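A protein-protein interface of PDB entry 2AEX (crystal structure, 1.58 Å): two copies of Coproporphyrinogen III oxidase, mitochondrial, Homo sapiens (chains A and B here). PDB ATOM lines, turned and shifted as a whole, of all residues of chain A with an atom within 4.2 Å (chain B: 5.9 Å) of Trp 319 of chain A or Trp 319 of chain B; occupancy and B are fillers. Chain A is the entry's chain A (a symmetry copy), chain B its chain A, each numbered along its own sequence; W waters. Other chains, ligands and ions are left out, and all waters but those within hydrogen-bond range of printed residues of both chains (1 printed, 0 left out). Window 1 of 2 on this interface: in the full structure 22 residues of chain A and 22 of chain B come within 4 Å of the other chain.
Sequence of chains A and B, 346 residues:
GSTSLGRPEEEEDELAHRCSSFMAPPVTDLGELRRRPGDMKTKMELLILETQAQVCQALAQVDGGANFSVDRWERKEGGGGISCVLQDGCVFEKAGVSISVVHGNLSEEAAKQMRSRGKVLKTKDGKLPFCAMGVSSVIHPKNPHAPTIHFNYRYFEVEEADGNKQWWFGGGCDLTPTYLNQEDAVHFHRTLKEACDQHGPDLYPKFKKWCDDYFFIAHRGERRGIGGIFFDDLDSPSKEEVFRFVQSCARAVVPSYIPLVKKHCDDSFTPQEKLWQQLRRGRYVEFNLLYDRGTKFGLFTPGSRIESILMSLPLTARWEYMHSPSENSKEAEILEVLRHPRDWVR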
ATOM      1  N   LYS A  94     -18.930   8.350  -9.750  1.00  0.00           N
ATOM      2  CA  LYS A  94     -18.536   7.160  -9.017  1.00  0.00           C
ATOM      3  C   LYS A  94     -18.633   7.478  -7.554  1.00  0.00           C
ATOM      4  O   LYS A  94     -18.194   8.533  -7.122  1.00  0.00           O
ATOM      5  CB  LYS A  94     -17.082   6.797  -9.296  1.00  0.00           C
ATOM      6  CG  LYS A  94     -16.793   6.148 -10.573  1.00  0.00           C
ATOM      7  CD  LYS A  94     -17.173   4.674 -10.567  1.00  0.00           C
ATOM      8  CE  LYS A  94     -16.501   3.971 -11.713  1.00  0.00           C
ATOM      9  NZ  LYS A  94     -15.058   3.680 -11.423  1.00  0.00           N
ATOM     10  N   GLY A 282      -6.962  12.280 -13.441  1.00  0.00           N
ATOM     11  CA  GLY A 282      -5.769  11.513 -13.800  1.00  0.00           C
ATOM     12  C   GLY A 282      -4.692  11.592 -12.729  1.00  0.00           C
ATOM     13  O   GLY A 282      -4.029  10.605 -12.413  1.00  0.00           O
ATOM     14  N   VAL A 285      -5.556   9.231  -9.886  1.00  0.00           N
ATOM     15  CA  VAL A 285      -5.206   7.867 -10.240  1.00  0.00           C
ATOM     16  C   VAL A 285      -3.688   7.642 -10.138  1.00  0.00           C
ATOM     17  O   VAL A 285      -3.245   6.602  -9.621  1.00  0.00           O
ATOM     18  CB  VAL A 285      -5.738   7.531 -11.643  1.00  0.00           C
ATOM     19  CG1 VAL A 285      -5.228   6.170 -12.119  1.00  0.00           C
ATOM     20  CG2 VAL A 285      -7.271   7.529 -11.647  1.00  0.00           C
ATOM     21  N   GLU A 286      -2.930   8.631 -10.595  1.00  0.00           N
ATOM     22  CA  GLU A 286      -1.466   8.572 -10.623  1.00  0.00           C
ATOM     23  C   GLU A 286      -0.856   8.422  -9.243  1.00  0.00           C
ATOM     24  O   GLU A 286       0.205   7.818  -9.078  1.00  0.00           O
ATOM     25  CB  GLU A 286      -0.947   9.833 -11.304  1.00  0.00           C
ATOM     26  CG  GLU A 286       0.426   9.784 -11.829  1.00  0.00           C
ATOM     27  CD  GLU A 286       0.786  11.050 -12.517  1.00  0.00           C
ATOM     28  OE1 GLU A 286       1.626  11.771 -11.976  1.00  0.00           O
ATOM     29  OE2 GLU A 286       0.196  11.350 -13.589  1.00  0.00           O
ATOM     30  N   LEU A 313     -11.128   4.390  -8.308  1.00  0.00           N
ATOM     31  CA  LEU A 313     -10.952   4.909  -9.640  1.00  0.00           C
ATOM     32  C   LEU A 313     -12.199   5.726 -10.041  1.00  0.00           C
ATOM     33  O   LEU A 313     -13.316   5.310  -9.765  1.00  0.00           O
ATOM     34  CB  LEU A 313     -10.740   3.747 -10.604  1.00  0.00           C
ATOM     35  CG  LEU A 313      -9.442   2.965 -10.349  1.00  0.00           C
ATOM     36  CD1 LEU A 313      -9.431   1.699 -11.134  1.00  0.00           C
ATOM     37  CD2 LEU A 313      -8.257   3.820 -10.676  1.00  0.00           C
ATOM     38  N   PRO A 314     -12.001   6.851 -10.747  1.00  0.00           N
ATOM     39  CA  PRO A 314     -13.139   7.640 -11.233  1.00  0.00           C
ATOM     40  C   PRO A 314     -13.777   6.957 -12.432  1.00  0.00           C
ATOM     41  O   PRO A 314     -13.347   5.876 -12.850  1.00  0.00           O
ATOM     42  CB  PRO A 314     -12.491   8.943 -11.616  1.00  0.00           C
ATOM     43  CG  PRO A 314     -11.135   8.551 -12.068  1.00  0.00           C
ATOM     44  CD  PRO A 314     -10.726   7.420 -11.208  1.00  0.00           C
ATOM     45  N   LEU A 315     -14.845   7.533 -12.945  1.00  0.00           N
ATOM     46  CA  LEU A 315     -15.461   7.018 -14.164  1.00  0.00           C
ATOM     47  C   LEU A 315     -14.531   7.263 -15.350  1.00  0.00           C
ATOM     48  O   LEU A 315     -14.316   6.358 -16.179  1.00  0.00           O
ATOM     49  CB  LEU A 315     -16.823   7.687 -14.377  1.00  0.00           C
ATOM     50  CG  LEU A 315     -17.654   7.073 -15.497  1.00  0.00           C
ATOM     51  CD1 LEU A 315     -18.020   5.630 -15.235  1.00  0.00           C
ATOM     52  CD2 LEU A 315     -18.881   7.894 -15.671  1.00  0.00           C
ATOM     53  N   ALA A 317     -10.808   9.662 -16.754  1.00  0.00           N
ATOM     54  CA  ALA A 317      -9.634  10.466 -16.454  1.00  0.00           C
ATOM     55  C   ALA A 317      -8.899  10.787 -17.736  1.00  0.00           C
ATOM     56  O   ALA A 317      -9.108  10.142 -18.772  1.00  0.00           O
ATOM     57  CB  ALA A 317      -8.695   9.754 -15.469  1.00  0.00           C
ATOM     58  N   ARG A 318      -8.018  11.767 -17.648  1.00  0.00           N
ATOM     59  CA  ARG A 318      -7.198  12.209 -18.761  1.00  0.00           C
ATOM     60  C   ARG A 318      -5.754  12.401 -18.311  1.00  0.00           C
ATOM     61  O   ARG A 318      -5.510  12.785 -17.172  1.00  0.00           O
ATOM     62  CB  ARG A 318      -7.728  13.538 -19.294  1.00  0.00           C
ATOM     63  CG  ARG A 318      -7.122  14.045 -20.568  1.00  0.00           C
ATOM     64  CD  ARG A 318      -7.671  15.415 -20.886  1.00  0.00           C
ATOM     65  NE  ARG A 318      -7.154  15.908 -22.154  1.00  0.00           N
ATOM     66  CZ  ARG A 318      -7.671  15.611 -23.345  1.00  0.00           C
ATOM     67  NH1 ARG A 318      -8.728  14.808 -23.456  1.00  0.00           N
ATOM     68  NH2 ARG A 318      -7.112  16.103 -24.438  1.00  0.00           N
ATOM     69  N   TRP A 319      -4.803  12.158 -19.210  1.00  0.00           N
ATOM     70  CA  TRP A 319      -3.387  12.398 -18.941  1.00  0.00           C
ATOM     71  C   TRP A 319      -2.788  13.078 -20.156  1.00  0.00           C
ATOM     72  O   TRP A 319      -2.894  12.569 -21.275  1.00  0.00           O
ATOM     73  CB  TRP A 319      -2.612  11.090 -18.635  1.00  0.00           C
ATOM     74  CG  TRP A 319      -3.106  10.345 -17.438  1.00  0.00           C
ATOM     75  CD1 TRP A 319      -2.740  10.519 -16.106  1.00  0.00           C
ATOM     76  CD2 TRP A 319      -4.069   9.307 -17.440  1.00  0.00           C
ATOM     77  NE1 TRP A 319      -3.442   9.659 -15.329  1.00  0.00           N
ATOM     78  CE2 TRP A 319      -4.263   8.900 -16.105  1.00  0.00           C
ATOM     79  CE3 TRP A 319      -4.799   8.681 -18.437  1.00  0.00           C
ATOM     80  CZ2 TRP A 319      -5.133   7.882 -15.768  1.00  0.00           C
ATOM     81  CZ3 TRP A 319      -5.670   7.689 -18.096  1.00  0.00           C
ATOM     82  CH2 TRP A 319      -5.830   7.297 -16.783  1.00  0.00           C
ATOM     83  N   GLU A 320      -2.189  14.245 -19.951  1.00  0.00           N
ATOM     84  CA  GLU A 320      -1.651  15.020 -21.067  1.00  0.00           C
ATOM     85  C   GLU A 320      -0.691  16.093 -20.576  1.00  0.00           C
ATOM     86  O   GLU A 320      -0.976  16.808 -19.600  1.00  0.00           O
ATOM     87  CB  GLU A 320      -2.795  15.585 -21.924  1.00  0.00           C
ATOM     88  CG  GLU A 320      -3.181  17.009 -21.768  1.00  0.00           C
ATOM     89  CD  GLU A 320      -4.240  17.386 -22.776  1.00  0.00           C
ATOM     90  OE1 GLU A 320      -4.073  17.051 -23.966  1.00  0.00           O
ATOM     91  OE2 GLU A 320      -5.238  18.009 -22.391  1.00  0.00           O
ATOM     92  N   GLN B  87       1.332  13.750 -28.852  1.00  0.00           N
ATOM     93  CA  GLN B  87       0.104  13.802 -28.101  1.00  0.00           C
ATOM     94  C   GLN B  87      -1.053  14.369 -28.914  1.00  0.00           C
ATOM     95  O   GLN B  87      -0.891  15.352 -29.641  1.00  0.00           O
ATOM     96  CB  GLN B  87       0.379  14.660 -26.880  1.00  0.00           C
ATOM     97  CG  GLN B  87      -0.752  14.891 -25.971  1.00  0.00           C
ATOM     98  CD  GLN B  87      -0.258  15.592 -24.741  1.00  0.00           C
ATOM     99  OE1 GLN B  87       0.299  14.962 -23.851  1.00  0.00           O
ATOM    100  NE2 GLN B  87      -0.415  16.911 -24.703  1.00  0.00           N
ATOM    101  N   LYS B  94      -1.771   9.222 -28.073  1.00  0.00           N
ATOM    102  CA  LYS B  94      -0.527   9.277 -27.325  1.00  0.00           C
ATOM    103  C   LYS B  94       0.445   8.353 -27.999  1.00  0.00           C
ATOM    104  O   LYS B  94       0.091   7.238 -28.353  1.00  0.00           O
ATOM    105  CB  LYS B  94      -0.715   8.763 -25.903  1.00  0.00           C
ATOM    106  CG  LYS B  94      -1.366   9.662 -24.953  1.00  0.00           C
ATOM    107  CD  LYS B  94      -0.422  10.746 -24.449  1.00  0.00           C
ATOM    108  CE  LYS B  94      -0.987  11.374 -23.206  1.00  0.00           C
ATOM    109  NZ  LYS B  94      -0.769  10.515 -21.996  1.00  0.00           N
ATOM    110  N   GLN B 278     -12.393   2.889 -24.314  1.00  0.00           N
ATOM    111  CA  GLN B 278     -12.047   3.592 -23.081  1.00  0.00           C
ATOM    112  C   GLN B 278     -11.946   2.642 -21.889  1.00  0.00           C
ATOM    113  O   GLN B 278     -11.033   2.775 -21.052  1.00  0.00           O
ATOM    114  CB  GLN B 278     -13.075   4.677 -22.819  1.00  0.00           C
ATOM    115  CG  GLN B 278     -13.026   5.748 -23.875  1.00  0.00           C
ATOM    116  CD  GLN B 278     -11.660   6.334 -23.998  1.00  0.00           C
ATOM    117  OE1 GLN B 278     -11.179   7.006 -23.079  1.00  0.00           O
ATOM    118  NE2 GLN B 278     -10.983   6.062 -25.117  1.00  0.00           N
ATOM    119  N   LEU B 279     -12.823   1.651 -21.821  1.00  0.00           N
ATOM    120  CA  LEU B 279     -12.740   0.635 -20.780  1.00  0.00           C
ATOM    121  C   LEU B 279     -11.477  -0.237 -20.950  1.00  0.00           C
ATOM    122  O   LEU B 279     -10.801  -0.584 -19.985  1.00  0.00           O
ATOM    123  CB  LEU B 279     -13.988  -0.234 -20.782  1.00  0.00           C
ATOM    124  CG  LEU B 279     -15.298   0.434 -20.408  1.00  0.00           C
ATOM    125  CD1 LEU B 279     -16.441  -0.491 -20.690  1.00  0.00           C
ATOM    126  CD2 LEU B 279     -15.250   0.832 -18.944  1.00  0.00           C
ATOM    127  N   ARG B 281      -8.696   0.770 -22.324  1.00  0.00           N
ATOM    128  CA  ARG B 281      -7.590   1.646 -21.958  1.00  0.00           C
ATOM    129  C   ARG B 281      -7.459   1.744 -20.420  1.00  0.00           C
ATOM    130  O   ARG B 281      -6.362   1.828 -19.874  1.00  0.00           O
ATOM    131  CB  ARG B 281      -7.817   3.025 -22.589  1.00  0.00           C
ATOM    132  CG  ARG B 281      -7.729   2.967 -24.135  1.00  0.00           C
ATOM    133  CD  ARG B 281      -6.294   3.055 -24.508  1.00  0.00           C
ATOM    134  NE  ARG B 281      -5.955   2.656 -25.882  1.00  0.00           N
ATOM    135  CZ  ARG B 281      -6.082   3.423 -26.963  1.00  0.00           C
ATOM    136  NH1 ARG B 281      -6.667   4.604 -26.914  1.00  0.00           N
ATOM    137  NH2 ARG B 281      -5.641   2.967 -28.125  1.00  0.00           N
ATOM    138  N   GLY B 282      -8.593   1.726 -19.732  1.00  0.00           N
ATOM    139  CA  GLY B 282      -8.566   1.648 -18.271  1.00  0.00           C
ATOM    140  C   GLY B 282      -7.910   0.367 -17.776  1.00  0.00           C
ATOM    141  O   GLY B 282      -7.152   0.369 -16.808  1.00  0.00           O
ATOM    142  N   ARG B 283      -8.175  -0.758 -18.457  1.00  0.00           N
ATOM    143  CA  ARG B 283      -7.474  -2.021 -18.124  1.00  0.00           C
ATOM    144  C   ARG B 283      -5.979  -1.902 -18.304  1.00  0.00           C
ATOM    145  O   ARG B 283      -5.201  -2.388 -17.508  1.00  0.00           O
ATOM    146  CB  ARG B 283      -7.968  -3.149 -19.011  1.00  0.00           C
ATOM    147  CG  ARG B 283      -9.342  -3.661 -18.663  1.00  0.00           C
ATOM    148  CD  ARG B 283      -9.346  -4.578 -17.480  1.00  0.00           C
ATOM    149  NE  ARG B 283     -10.503  -5.464 -17.580  1.00  0.00           N
ATOM    150  CZ  ARG B 283     -11.742  -5.169 -17.200  1.00  0.00           C
ATOM    151  NH1 ARG B 283     -12.016  -4.011 -16.624  1.00  0.00           N
ATOM    152  NH2 ARG B 283     -12.713  -6.069 -17.370  1.00  0.00           N
ATOM    153  N   VAL B 285      -4.137   0.713 -17.991  1.00  0.00           N
ATOM    154  CA  VAL B 285      -3.638   1.488 -16.869  1.00  0.00           C
ATOM    155  C   VAL B 285      -3.618   0.647 -15.582  1.00  0.00           C
ATOM    156  O   VAL B 285      -2.640   0.703 -14.815  1.00  0.00           O
ATOM    157  CB  VAL B 285      -4.470   2.770 -16.699  1.00  0.00           C
ATOM    158  CG1 VAL B 285      -4.089   3.513 -15.418  1.00  0.00           C
ATOM    159  CG2 VAL B 285      -4.274   3.698 -17.904  1.00  0.00           C
ATOM    160  N   GLU B 286      -4.672  -0.137 -15.393  1.00  0.00           N
ATOM    161  CA  GLU B 286      -4.848  -0.970 -14.200  1.00  0.00           C
ATOM    162  C   GLU B 286      -3.750  -2.004 -14.037  1.00  0.00           C
ATOM    163  O   GLU B 286      -3.393  -2.383 -12.920  1.00  0.00           O
ATOM    164  CB  GLU B 286      -6.211  -1.646 -14.283  1.00  0.00           C
ATOM    165  CG  GLU B 286      -6.772  -2.160 -13.023  1.00  0.00           C
ATOM    166  CD  GLU B 286      -8.124  -2.739 -13.232  1.00  0.00           C
ATOM    167  OE1 GLU B 286      -8.242  -3.959 -13.120  1.00  0.00           O
ATOM    168  OE2 GLU B 286      -9.072  -1.972 -13.550  1.00  0.00           O
ATOM    169  N   LEU B 289      -1.352  -0.061 -12.137  1.00  0.00           N
ATOM    170  CA  LEU B 289      -1.935   0.309 -10.832  1.00  0.00           C
ATOM    171  C   LEU B 289      -1.853  -0.810  -9.798  1.00  0.00           C
ATOM    172  O   LEU B 289      -1.543  -0.579  -8.618  1.00  0.00           O
ATOM    173  CB  LEU B 289      -3.405   0.697 -11.009  1.00  0.00           C
ATOM    174  CG  LEU B 289      -3.717   2.117 -11.443  1.00  0.00           C
ATOM    175  CD1 LEU B 289      -5.162   2.274 -11.833  1.00  0.00           C
ATOM    176  CD2 LEU B 289      -3.403   3.049 -10.277  1.00  0.00           C
ATOM    177  N   LEU B 313       0.746   6.032 -20.191  1.00  0.00           N
ATOM    178  CA  LEU B 313      -0.638   6.349 -19.950  1.00  0.00           C
ATOM    179  C   LEU B 313      -1.286   6.845 -21.262  1.00  0.00           C
ATOM    180  O   LEU B 313      -0.673   7.611 -21.993  1.00  0.00           O
ATOM    181  CB  LEU B 313      -0.723   7.424 -18.872  1.00  0.00           C
ATOM    182  CG  LEU B 313      -0.218   6.955 -17.498  1.00  0.00           C
ATOM    183  CD1 LEU B 313      -0.073   8.113 -16.572  1.00  0.00           C
ATOM    184  CD2 LEU B 313      -1.144   5.921 -16.937  1.00  0.00           C
ATOM    185  N   PRO B 314      -2.546   6.457 -21.515  1.00  0.00           N
ATOM    186  CA  PRO B 314      -3.258   6.949 -22.700  1.00  0.00           C
ATOM    187  C   PRO B 314      -3.706   8.385 -22.483  1.00  0.00           C
ATOM    188  O   PRO B 314      -3.438   8.983 -21.435  1.00  0.00           O
ATOM    189  CB  PRO B 314      -4.429   6.009 -22.791  1.00  0.00           C
ATOM    190  CG  PRO B 314      -4.723   5.665 -21.379  1.00  0.00           C
ATOM    191  CD  PRO B 314      -3.417   5.607 -20.689  1.00  0.00           C
ATOM    192  N   LEU B 315      -4.319   8.974 -23.489  1.00  0.00           N
ATOM    193  CA  LEU B 315      -4.889  10.310 -23.340  1.00  0.00           C
ATOM    194  C   LEU B 315      -6.090  10.254 -22.400  1.00  0.00           C
ATOM    195  O   LEU B 315      -6.223  11.103 -21.497  1.00  0.00           O
ATOM    196  CB  LEU B 315      -5.284  10.860 -24.715  1.00  0.00           C
ATOM    197  CG  LEU B 315      -5.687  12.329 -24.711  1.00  0.00           C
ATOM    198  CD1 LEU B 315      -4.563  13.246 -24.287  1.00  0.00           C
ATOM    199  CD2 LEU B 315      -6.161  12.687 -26.074  1.00  0.00           C
ATOM    200  N   THR B 316      -6.942   9.251 -22.563  1.00  0.00           N
ATOM    201  CA  THR B 316      -8.116   9.088 -21.729  1.00  0.00           C
ATOM    202  C   THR B 316      -8.378   7.616 -21.447  1.00  0.00           C
ATOM    203  O   THR B 316      -7.877   6.715 -22.149  1.00  0.00           O
ATOM    204  CB  THR B 316      -9.371   9.682 -22.377  1.00  0.00           C
ATOM    205  OG1 THR B 316      -9.633   9.017 -23.628  1.00  0.00           O
ATOM    206  CG2 THR B 316      -9.202  11.185 -22.602  1.00  0.00           C
ATOM    207  N   ALA B 317      -9.122   7.377 -20.373  1.00  0.00           N
ATOM    208  CA  ALA B 317      -9.523   6.037 -19.974  1.00  0.00           C
ATOM    209  C   ALA B 317     -10.820   6.106 -19.200  1.00  0.00           C
ATOM    210  O   ALA B 317     -11.220   7.172 -18.713  1.00  0.00           O
ATOM    211  CB  ALA B 317      -8.440   5.347 -19.131  1.00  0.00           C
ATOM    212  N   ARG B 318     -11.456   4.955 -19.066  1.00  0.00           N
ATOM    213  CA  ARG B 318     -12.705   4.810 -18.340  1.00  0.00           C
ATOM    214  C   ARG B 318     -12.654   3.582 -17.439  1.00  0.00           C
ATOM    215  O   ARG B 318     -12.021   2.590 -17.785  1.00  0.00           O
ATOM    216  CB  ARG B 318     -13.858   4.648 -19.328  1.00  0.00           C
ATOM    217  CG  ARG B 318     -15.245   4.682 -18.759  1.00  0.00           C
ATOM    218  CD  ARG B 318     -16.251   4.390 -19.846  1.00  0.00           C
ATOM    219  NE  ARG B 318     -17.613   4.482 -19.342  1.00  0.00           N
ATOM    220  CZ  ARG B 318     -18.304   5.617 -19.242  1.00  0.00           C
ATOM    221  NH1 ARG B 318     -17.770   6.782 -19.604  1.00  0.00           N
ATOM    222  NH2 ARG B 318     -19.534   5.589 -18.755  1.00  0.00           N
ATOM    223  N   TRP B 319     -13.337   3.640 -16.299  1.00  0.00           N
ATOM    224  CA  TRP B 319     -13.453   2.499 -15.393  1.00  0.00           C
ATOM    225  C   TRP B 319     -14.896   2.404 -14.941  1.00  0.00           C
ATOM    226  O   TRP B 319     -15.456   3.374 -14.423  1.00  0.00           O
ATOM    227  CB  TRP B 319     -12.523   2.625 -14.158  1.00  0.00           C
ATOM    228  CG  TRP B 319     -11.068   2.704 -14.487  1.00  0.00           C
ATOM    229  CD1 TRP B 319     -10.172   1.655 -14.679  1.00  0.00           C
ATOM    230  CD2 TRP B 319     -10.319   3.890 -14.678  1.00  0.00           C
ATOM    231  NE1 TRP B 319      -8.951   2.156 -14.986  1.00  0.00           N
ATOM    232  CE2 TRP B 319      -8.998   3.516 -14.995  1.00  0.00           C
ATOM    233  CE3 TRP B 319     -10.631   5.239 -14.623  1.00  0.00           C
ATOM    234  CZ2 TRP B 319      -8.005   4.450 -15.222  1.00  0.00           C
ATOM    235  CZ3 TRP B 319      -9.651   6.155 -14.866  1.00  0.00           C
ATOM    236  CH2 TRP B 319      -8.361   5.764 -15.158  1.00  0.00           C
ATOM    237  N   GLU B 320     -15.517   1.252 -15.165  1.00  0.00           N
ATOM    238  CA  GLU B 320     -16.932   1.085 -14.842  1.00  0.00           C
ATOM    239  C   GLU B 320     -17.318  -0.386 -14.814  1.00  0.00           C
ATOM    240  O   GLU B 320     -16.944  -1.162 -15.710  1.00  0.00           O
ATOM    241  CB  GLU B 320     -17.800   1.914 -15.802  1.00  0.00           C
ATOM    242  CG  GLU B 320     -18.487   1.233 -16.927  1.00  0.00           C
ATOM    243  CD  GLU B 320     -19.371   2.202 -17.675  1.00  0.00           C
ATOM    244  OE1 GLU B 320     -20.126   2.946 -17.017  1.00  0.00           O
ATOM    245  OE2 GLU B 320     -19.315   2.233 -18.911  1.00  0.00           O
ATOM    246  N   TYR B 321     -18.035  -0.762 -13.753  1.00  0.00           N
ATOM    247  CA  TYR B 321     -18.428  -2.152 -13.511  1.00  0.00           C
ATOM    248  C   TYR B 321     -19.500  -2.499 -14.528  1.00  0.00           C
ATOM    249  O   TYR B 321     -20.490  -1.773 -14.693  1.00  0.00           O
ATOM    250  CB  TYR B 321     -18.933  -2.373 -12.079  1.00  0.00           C
ATOM    251  CG  TYR B 321     -18.222  -1.533 -11.028  1.00  0.00           C
ATOM    252  CD1 TYR B 321     -18.783  -0.336 -10.587  1.00  0.00           C
ATOM    253  CD2 TYR B 321     -17.003  -1.924 -10.473  1.00  0.00           C
ATOM    254  CE1 TYR B 321     -18.157   0.469  -9.647  1.00  0.00           C
ATOM    255  CE2 TYR B 321     -16.363  -1.118  -9.497  1.00  0.00           C
ATOM    256  CZ  TYR B 321     -16.959   0.083  -9.088  1.00  0.00           C
ATOM    257  OH  TYR B 321     -16.376   0.912  -8.132  1.00  0.00           O
HETATM  258  O   HOH W   1     -14.257   2.735  -9.016  1.00  0.00           O
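Trp 319 of chain A touches just these residues of chain B: Lys 94, Leu 313, Pro 314, Leu 315, Ala 317 and Trp 319. Trp 319 of chain B touches six residues of chain A. Of the printed residues of chain B, Leu 313 of chain A touches Leu 289 (3.6 Å) and Trp 319 (3.6 Å). Of the printed residues of chain B, Pro 314 of chain A touches Trp 319. Of the printed residues of chain B, Lys 94 of chain A touches Trp 319. Of the printed residues of chain A, Leu 289 of chain B touches Val 285 (3.6 Å) and Leu 313 (3.6 Å). The nearest residue of chain B that does not touch Trp 319 of chain A is Val 285 of chain B (4.1 Å). The nearest residue of chain A that does not touch Trp 319 of chain B is Val 285 of chain A (4.1 Å). The nearest printed residue of chain A that does not touch Leu 289 of chain B is Glu 286 of chain A (5.6 Å).
Hydrophobic or aromatic side chains of chain B within 4 Å of the printed part of chain A: Leu 289, Leu 313, Pro 314, Leu 315, Ala 317 and Trp 319. Among the printed residues, 21 pairs touch across the chains. Among the printed residues, no Asp or Glu carboxylate lies within 4 Å of a Lys or Arg side-chain nitrogen of the other chain.
Among the printed residues, merely in contact across the chains: Val 285 of chain A with Leu 289 of chain B, Leu 313 of chain A with Leu 289 of chain B, Leu 313 of chain A with Trp 319 of chain B, Pro 314 of chain A with Trp 319 of chain B, Leu 315 of chain A with Arg 318 of chain B, Leu 315 of chain A with Glu 320 of chain B, Ala 317 of chain A with Thr 316 of chain B, Ala 317 of chain A with Trp 319 of chain B, Arg 318 of chain A with Leu 315 of chain B, Arg 318 of chain A with Thr 316 of chain B, Trp 319 of chain A with Leu 313 of chain B, Trp 319 of chain A with Pro 314 of chain B, Trp 319 of chain A with Ala 317 of chain B, Trp 319 of chain A with Trp 319 of chain B, Glu 320 of chain A with Gln 87 of chain B and Glu 320 of chain A with Leu 315 of chain B.
N of Trp 319 of chain B sits at hydrogen-bond distance from O of Leu 315 of chain A, 2.9 Å away. O of Trp 319 of chain B lies close to NZ of Lys 94 of chain A (3.0 Å). The backbone NH (N) of Trp 319 of chain A lies within hydrogen-bond range of the backbone carbonyl oxygen (O) of Leu 315 of chain B, 2.9 Å away. O of Ala 317 of chain A is in hydrogen-bond range of N of Ala 317 of chain B, at 3.2 Å. O of Trp 319 of chain A lies close to NZ of Lys 94 of chain B.
Pro 314 of chain A touches Trp 319 of chain B, and with the chains exchanged Trp 319 of chain A touches Pro 314 of chain B. Leu 315 of chain A touches Glu 320 of chain B, and with the chains exchanged Glu 320 of chain A touches Leu 315 of chain B. Ala 317 of chain A touches Trp 319 of chain B, and with the chains exchanged Trp 319 of chain A touches Ala 317 of chain B. Trp 319 of chain A touches its own counterpart, Trp 319 of chain B. Of the 21 pairs that touch across the chains among the printed residues, 16 have their exchanged pair printed and touching as well.
Water W1 lies within hydrogen-bond range of the side-chain amino group of Lys 94 of chain A, the backbone carbonyl oxygen of Leu 313 of chain A and the side-chain hydroxyl of Tyr 321 of chain B.
NZ of Lys 94 of chain A sits at hydrogen-bond distance from O of Leu 313 of chain A, at 2.9 Å. N of Ala 317 of chain B is in hydrogen-bond range of OE1 of Gln 278 of chain B (3.4 Å). O of Gln 278 of chain B lies within hydrogen-bond range of N of Arg 318 of chain B, at 3.0 Å. The indole nitrogen of Trp 319 of chain A is in hydrogen-bond range of the backbone carbonyl oxygen of Gly 282 of chain A. OG1 of Thr 316 of chain B sits at hydrogen-bond distance from OE1 of Gln 278 of chain B (2.6 Å). NE of Arg 318 of chain B lies within salt-bridge range of OE2 of Glu 320 of chain B (2.9 Å).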
